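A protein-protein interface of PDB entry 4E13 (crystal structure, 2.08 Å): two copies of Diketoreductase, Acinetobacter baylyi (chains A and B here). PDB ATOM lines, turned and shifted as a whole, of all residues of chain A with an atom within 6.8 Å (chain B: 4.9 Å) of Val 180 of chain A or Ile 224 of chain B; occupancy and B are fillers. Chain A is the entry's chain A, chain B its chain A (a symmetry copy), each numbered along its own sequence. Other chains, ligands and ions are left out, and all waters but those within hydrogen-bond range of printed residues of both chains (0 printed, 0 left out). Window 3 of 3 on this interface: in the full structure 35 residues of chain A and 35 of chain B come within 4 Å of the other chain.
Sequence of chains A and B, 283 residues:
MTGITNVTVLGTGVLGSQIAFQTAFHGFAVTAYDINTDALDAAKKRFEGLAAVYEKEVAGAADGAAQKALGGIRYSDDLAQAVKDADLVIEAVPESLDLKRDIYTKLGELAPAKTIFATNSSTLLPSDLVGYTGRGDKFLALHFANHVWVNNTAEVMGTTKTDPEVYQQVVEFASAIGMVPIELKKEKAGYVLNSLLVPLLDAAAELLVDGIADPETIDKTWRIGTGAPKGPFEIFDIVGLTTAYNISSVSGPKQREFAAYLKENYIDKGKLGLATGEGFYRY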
ATOM      1  N   VAL A 150     -24.552  27.253 -22.700  1.00  0.00           N
ATOM      2  CA  VAL A 150     -24.253  28.250 -23.734  1.00  0.00           C
ATOM      3  C   VAL A 150     -22.744  28.374 -24.026  1.00  0.00           C
ATOM      4  O   VAL A 150     -22.334  28.587 -25.171  1.00  0.00           O
ATOM      5  CB  VAL A 150     -24.834  29.630 -23.367  1.00  0.00           C
ATOM      6  CG1 VAL A 150     -24.235  30.130 -22.063  1.00  0.00           C
ATOM      7  CG2 VAL A 150     -24.589  30.614 -24.493  1.00  0.00           C
ATOM      8  N   ASN A 151     -21.904  28.253 -23.004  1.00  0.00           N
ATOM      9  CA  ASN A 151     -20.466  28.161 -23.255  1.00  0.00           C
ATOM     10  C   ASN A 151     -20.167  26.663 -23.346  1.00  0.00           C
ATOM     11  O   ASN A 151     -19.639  26.058 -22.404  1.00  0.00           O
ATOM     12  CB  ASN A 151     -19.699  28.798 -22.093  1.00  0.00           C
ATOM     13  CG  ASN A 151     -20.128  30.234 -21.835  1.00  0.00           C
ATOM     14  OD1 ASN A 151     -20.454  30.606 -20.703  1.00  0.00           O
ATOM     15  ND2 ASN A 151     -20.124  31.052 -22.886  1.00  0.00           N
ATOM     16  N   ASN A 152     -20.529  26.070 -24.479  1.00  0.00           N
ATOM     17  CA  ASN A 152     -20.621  24.616 -24.566  1.00  0.00           C
ATOM     18  C   ASN A 152     -19.374  23.923 -25.113  1.00  0.00           C
ATOM     19  O   ASN A 152     -19.474  23.032 -25.961  1.00  0.00           O
ATOM     20  CB  ASN A 152     -21.852  24.201 -25.372  1.00  0.00           C
ATOM     21  CG  ASN A 152     -21.835  24.743 -26.786  1.00  0.00           C
ATOM     22  OD1 ASN A 152     -21.456  25.893 -27.030  1.00  0.00           O
ATOM     23  ND2 ASN A 152     -22.236  23.912 -27.728  1.00  0.00           N
ATOM     24  N   THR A 153     -18.202  24.316 -24.623  1.00  0.00           N
ATOM     25  CA  THR A 153     -16.978  23.589 -24.960  1.00  0.00           C
ATOM     26  C   THR A 153     -16.695  22.532 -23.902  1.00  0.00           C
ATOM     27  O   THR A 153     -17.044  22.692 -22.728  1.00  0.00           O
ATOM     28  CB  THR A 153     -15.763  24.511 -25.039  1.00  0.00           C
ATOM     29  OG1 THR A 153     -15.658  25.244 -23.813  1.00  0.00           O
ATOM     30  CG2 THR A 153     -15.883  25.473 -26.213  1.00  0.00           C
ATOM     31  N   ALA A 154     -16.063  21.447 -24.333  1.00  0.00           N
ATOM     32  CA  ALA A 154     -15.606  20.417 -23.423  1.00  0.00           C
ATOM     33  C   ALA A 154     -14.202  20.007 -23.855  1.00  0.00           C
ATOM     34  O   ALA A 154     -14.033  19.283 -24.841  1.00  0.00           O
ATOM     35  CB  ALA A 154     -16.549  19.227 -23.460  1.00  0.00           C
ATOM     36  N   GLU A 155     -13.204  20.505 -23.131  1.00  0.00           N
ATOM     37  CA  GLU A 155     -11.800  20.193 -23.406  1.00  0.00           C
ATOM     38  C   GLU A 155     -11.441  18.789 -22.941  1.00  0.00           C
ATOM     39  O   GLU A 155     -11.537  18.473 -21.752  1.00  0.00           O
ATOM     40  CB  GLU A 155     -10.900  21.243 -22.762  1.00  0.00           C
ATOM     41  CG  GLU A 155     -11.085  22.609 -23.404  1.00  0.00           C
ATOM     42  CD  GLU A 155     -10.333  23.732 -22.710  1.00  0.00           C
ATOM     43  OE1 GLU A 155     -10.465  23.882 -21.472  1.00  0.00           O
ATOM     44  OE2 GLU A 155      -9.604  24.469 -23.406  1.00  0.00           O
ATOM     45  N   ALA A 174     -19.205  13.833 -25.432  1.00  0.00           N
ATOM     46  CA  ALA A 174     -19.241  15.284 -25.420  1.00  0.00           C
ATOM     47  C   ALA A 174     -20.176  15.827 -26.509  1.00  0.00           C
ATOM     48  O   ALA A 174     -20.997  16.712 -26.244  1.00  0.00           O
ATOM     49  CB  ALA A 174     -17.837  15.846 -25.569  1.00  0.00           C
ATOM     50  N   SER A 175     -20.071  15.290 -27.724  1.00  0.00           N
ATOM     51  CA  SER A 175     -20.984  15.680 -28.803  1.00  0.00           C
ATOM     52  C   SER A 175     -22.418  15.303 -28.483  1.00  0.00           C
ATOM     53  O   SER A 175     -23.341  16.081 -28.744  1.00  0.00           O
ATOM     54  CB  SER A 175     -20.585  15.034 -30.131  1.00  0.00           C
ATOM     55  OG  SER A 175     -19.324  15.511 -30.565  1.00  0.00           O
ATOM     56  N   GLY A 178     -24.228  17.697 -26.525  1.00  0.00           N
ATOM     57  CA  GLY A 178     -24.326  19.018 -27.125  1.00  0.00           C
ATOM     58  C   GLY A 178     -23.134  19.924 -26.903  1.00  0.00           C
ATOM     59  O   GLY A 178     -23.261  21.146 -26.979  1.00  0.00           O
ATOM     60  N   MET A 179     -21.978  19.347 -26.610  1.00  0.00           N
ATOM     61  CA  MET A 179     -20.777  20.146 -26.403  1.00  0.00           C
ATOM     62  C   MET A 179     -19.956  20.212 -27.687  1.00  0.00           C
ATOM     63  O   MET A 179     -20.088  19.355 -28.565  1.00  0.00           O
ATOM     64  CB  MET A 179     -19.917  19.530 -25.293  1.00  0.00           C
ATOM     65  CG  MET A 179     -20.599  19.433 -23.932  1.00  0.00           C
ATOM     66  SD  MET A 179     -20.989  21.049 -23.233  1.00  0.00           S
ATOM     67  CE  MET A 179     -22.758  21.083 -23.483  1.00  0.00           C
ATOM     68  N   VAL A 180     -19.111  21.230 -27.794  1.00  0.00           N
ATOM     69  CA  VAL A 180     -18.088  21.255 -28.827  1.00  0.00           C
ATOM     70  C   VAL A 180     -16.810  20.657 -28.249  1.00  0.00           C
ATOM     71  O   VAL A 180     -16.148  21.280 -27.410  1.00  0.00           O
ATOM     72  CB  VAL A 180     -17.813  22.686 -29.303  1.00  0.00           C
ATOM     73  CG1 VAL A 180     -16.655  22.705 -30.292  1.00  0.00           C
ATOM     74  CG2 VAL A 180     -19.066  23.252 -29.965  1.00  0.00           C
ATOM     75  N   PRO A 181     -16.451  19.433 -28.679  1.00  0.00           N
ATOM     76  CA  PRO A 181     -15.230  18.814 -28.150  1.00  0.00           C
ATOM     77  C   PRO A 181     -13.972  19.593 -28.540  1.00  0.00           C
ATOM     78  O   PRO A 181     -13.724  19.847 -29.722  1.00  0.00           O
ATOM     79  CB  PRO A 181     -15.217  17.431 -28.812  1.00  0.00           C
ATOM     80  CG  PRO A 181     -16.644  17.156 -29.151  1.00  0.00           C
ATOM     81  CD  PRO A 181     -17.206  18.506 -29.542  1.00  0.00           C
ATOM     82  N   ILE A 182     -13.188  19.990 -27.548  1.00  0.00           N
ATOM     83  CA  ILE A 182     -11.887  20.584 -27.809  1.00  0.00           C
ATOM     84  C   ILE A 182     -10.842  19.532 -27.479  1.00  0.00           C
ATOM     85  O   ILE A 182     -10.603  19.242 -26.303  1.00  0.00           O
ATOM     86  CB  ILE A 182     -11.676  21.860 -26.966  1.00  0.00           C
ATOM     87  CG1 ILE A 182     -12.738  22.900 -27.340  1.00  0.00           C
ATOM     88  CG2 ILE A 182     -10.283  22.426 -27.163  1.00  0.00           C
ATOM     89  CD1 ILE A 182     -12.819  23.143 -28.838  1.00  0.00           C
ATOM     90  N   GLU A 183     -10.248  18.935 -28.508  1.00  0.00           N
ATOM     91  CA  GLU A 183      -9.366  17.786 -28.313  1.00  0.00           C
ATOM     92  C   GLU A 183      -7.896  18.157 -28.118  1.00  0.00           C
ATOM     93  O   GLU A 183      -7.216  18.515 -29.082  1.00  0.00           O
ATOM     94  CB  GLU A 183      -9.485  16.837 -29.492  1.00  0.00           C
ATOM     95  CG  GLU A 183     -10.895  16.374 -29.764  1.00  0.00           C
ATOM     96  CD  GLU A 183     -10.948  15.375 -30.893  1.00  0.00           C
ATOM     97  OE1 GLU A 183      -9.868  14.910 -31.308  1.00  0.00           O
ATOM     98  OE2 GLU A 183     -12.057  15.065 -31.379  1.00  0.00           O
ATOM     99  N   LEU A 193      -8.241  26.994 -23.628  1.00  0.00           N
ATOM    100  CA  LEU A 193      -8.858  28.304 -23.423  1.00  0.00           C
ATOM    101  C   LEU A 193      -8.132  29.175 -22.406  1.00  0.00           C
ATOM    102  O   LEU A 193      -7.800  30.330 -22.695  1.00  0.00           O
ATOM    103  CB  LEU A 193     -10.347  28.187 -23.067  1.00  0.00           C
ATOM    104  CG  LEU A 193     -11.024  29.541 -22.831  1.00  0.00           C
ATOM    105  CD1 LEU A 193     -10.759  30.481 -24.005  1.00  0.00           C
ATOM    106  CD2 LEU A 193     -12.517  29.361 -22.596  1.00  0.00           C
ATOM    107  N   LYS B 220     -11.012  27.713 -32.858  1.00  0.00           N
ATOM    108  CA  LYS B 220     -12.413  27.604 -32.462  1.00  0.00           C
ATOM    109  C   LYS B 220     -12.571  27.783 -30.954  1.00  0.00           C
ATOM    110  O   LYS B 220     -13.582  28.321 -30.491  1.00  0.00           O
ATOM    111  CB  LYS B 220     -13.068  26.303 -32.936  1.00  0.00           C
ATOM    112  CG  LYS B 220     -12.626  25.036 -32.246  1.00  0.00           C
ATOM    113  CD  LYS B 220     -13.391  23.858 -32.844  1.00  0.00           C
ATOM    114  CE  LYS B 220     -12.982  22.522 -32.235  1.00  0.00           C
ATOM    115  NZ  LYS B 220     -13.684  21.390 -32.914  1.00  0.00           N
ATOM    116  N   THR B 221     -11.567  27.360 -30.185  1.00  0.00           N
ATOM    117  CA  THR B 221     -11.615  27.536 -28.743  1.00  0.00           C
ATOM    118  C   THR B 221     -11.652  29.021 -28.396  1.00  0.00           C
ATOM    119  O   THR B 221     -12.361  29.440 -27.479  1.00  0.00           O
ATOM    120  CB  THR B 221     -10.399  26.885 -28.039  1.00  0.00           C
ATOM    121  OG1 THR B 221     -10.401  25.477 -28.284  1.00  0.00           O
ATOM    122  CG2 THR B 221     -10.452  27.142 -26.540  1.00  0.00           C
ATOM    123  N   TRP B 222     -10.884  29.825 -29.121  1.00  0.00           N
ATOM    124  CA  TRP B 222     -10.851  31.249 -28.843  1.00  0.00           C
ATOM    125  C   TRP B 222     -12.159  31.923 -29.281  1.00  0.00           C
ATOM    126  O   TRP B 222     -12.711  32.743 -28.540  1.00  0.00           O
ATOM    127  CB  TRP B 222      -9.676  31.914 -29.552  1.00  0.00           C
ATOM    128  CG  TRP B 222      -9.513  33.355 -29.181  1.00  0.00           C
ATOM    129  CD1 TRP B 222      -9.726  34.449 -29.986  1.00  0.00           C
ATOM    130  CD2 TRP B 222      -9.096  33.874 -27.907  1.00  0.00           C
ATOM    131  NE1 TRP B 222      -9.461  35.609 -29.292  1.00  0.00           N
ATOM    132  CE2 TRP B 222      -9.074  35.287 -28.018  1.00  0.00           C
ATOM    133  CE3 TRP B 222      -8.737  33.281 -26.681  1.00  0.00           C
ATOM    134  CZ2 TRP B 222      -8.708  36.118 -26.951  1.00  0.00           C
ATOM    135  CZ3 TRP B 222      -8.373  34.103 -25.626  1.00  0.00           C
ATOM    136  CH2 TRP B 222      -8.361  35.510 -25.767  1.00  0.00           C
ATOM    137  N   ARG B 223     -12.645  31.600 -30.480  1.00  0.00           N
ATOM    138  CA  ARG B 223     -13.874  32.230 -30.971  1.00  0.00           C
ATOM    139  C   ARG B 223     -15.063  31.901 -30.067  1.00  0.00           C
ATOM    140  O   ARG B 223     -15.824  32.793 -29.678  1.00  0.00           O
ATOM    141  CB  ARG B 223     -14.173  31.838 -32.422  1.00  0.00           C
ATOM    142  CG  ARG B 223     -13.142  32.328 -33.428  1.00  0.00           C
ATOM    143  CD  ARG B 223     -13.665  32.132 -34.850  1.00  0.00           C
ATOM    144  NE  ARG B 223     -14.082  30.749 -35.053  1.00  0.00           N
ATOM    145  CZ  ARG B 223     -13.287  29.795 -35.527  1.00  0.00           C
ATOM    146  NH1 ARG B 223     -12.028  30.077 -35.855  1.00  0.00           N
ATOM    147  NH2 ARG B 223     -13.748  28.555 -35.672  1.00  0.00           N
ATOM    148  N   ILE B 224     -15.191  30.633 -29.699  1.00  0.00           N
ATOM    149  CA  ILE B 224     -16.287  30.182 -28.846  1.00  0.00           C
ATOM    150  C   ILE B 224     -16.145  30.721 -27.428  1.00  0.00           C
ATOM    151  O   ILE B 224     -17.120  31.178 -26.824  1.00  0.00           O
ATOM    152  CB  ILE B 224     -16.339  28.652 -28.801  1.00  0.00           C
ATOM    153  CG1 ILE B 224     -16.712  28.103 -30.173  1.00  0.00           C
ATOM    154  CG2 ILE B 224     -17.280  28.174 -27.720  1.00  0.00           C
ATOM    155  CD1 ILE B 224     -16.721  26.584 -30.244  1.00  0.00           C
ATOM    156  N   GLY B 225     -14.925  30.681 -26.908  1.00  0.00           N
ATOM    157  CA  GLY B 225     -14.695  31.095 -25.536  1.00  0.00           C
ATOM    158  C   GLY B 225     -14.763  32.584 -25.278  1.00  0.00           C
ATOM    159  O   GLY B 225     -15.130  33.014 -24.179  1.00  0.00           O
ATOM    160  N   THR B 226     -14.405  33.392 -26.267  1.00  0.00           N
ATOM    161  CA  THR B 226     -14.431  34.835 -26.077  1.00  0.00           C
ATOM    162  C   THR B 226     -15.451  35.521 -26.978  1.00  0.00           C
ATOM    163  O   THR B 226     -15.731  36.711 -26.815  1.00  0.00           O
ATOM    164  CB  THR B 226     -13.058  35.458 -26.346  1.00  0.00           C
ATOM    165  OG1 THR B 226     -12.685  35.211 -27.708  1.00  0.00           O
ATOM    166  CG2 THR B 226     -12.015  34.857 -25.418  1.00  0.00           C
ATOM    167  N   GLY B 227     -15.990  34.780 -27.936  1.00  0.00           N
ATOM    168  CA  GLY B 227     -16.884  35.385 -28.905  1.00  0.00           C
ATOM    169  C   GLY B 227     -16.163  36.193 -29.965  1.00  0.00           C
ATOM    170  O   GLY B 227     -16.802  36.896 -30.754  1.00  0.00           O
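The backbone carbonyl oxygen (O) of Asn 152 of chain A lies within hydrogen-bond range of the backbone NH (N) of Val 180 of chain A (2.6 Å).
The backbone NH (N) of Ala 154 of chain A sits at hydrogen-bond distance from the backbone carbonyl oxygen (O) of Val 180 of chain A.
The backbone carbonyl oxygen of Ala 154 of chain A is in hydrogen-bond range of the backbone NH of Ile 182 of chain A.
The side-chain carboxylate of Glu 155 of chain A is in hydrogen-bond range of the backbone NH of Leu 193 of chain A (2.9 Å).
Val 180 of chain A touches just one residue of chain B: Ile 224 (3.9 Å).
Ile 224 of chain B touches just these residues of chain A: Thr 153 (3.4 Å) and Val 180 (3.9 Å).
Printed residues of chain B within 4 Å of Ile 182 of chain A: Lys 220 (3.5 Å) and Thr 221 (3.3 Å).
Printed residues of chain B within 4 Å of Leu 193 of chain A: Thr 221.
Of the printed residues of chain B, Thr 153 of chain A touches Ile 224.
The nearest residue of chain B that does not touch Val 180 of chain A is Lys 220 of chain B (4.2 Å).
No position is printed for both chains.
Of the 6 pairs that touch across the chains among the printed residues, none has its exchanged pair printed and touching as well.
Of the 15 printed residues of chain A, 5 touch a printed residue of chain B.
Hydrophobic or aromatic side chains of chain A within 4 Å of the printed part of chain B: Val 180, Ile 182 and Leu 193.
Among the printed residues, 6 pairs touch across the chains.
Among the printed residues, no Asp or Glu carboxylate lies within 4 Å of a Lys or Arg side-chain nitrogen of the other chain.
Among the printed residues, merely in contact across the chains: Thr 153 of chain A with Ile 224 of chain B, Val 180 of chain A with Ile 224 of chain B, Pro 181 of chain A with Lys 220 of chain B, Ile 182 of chain A with Lys 220 of chain B, Ile 182 of chain A with Thr 221 of chain B and Leu 193 of chain A with Thr 221 of chain B.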
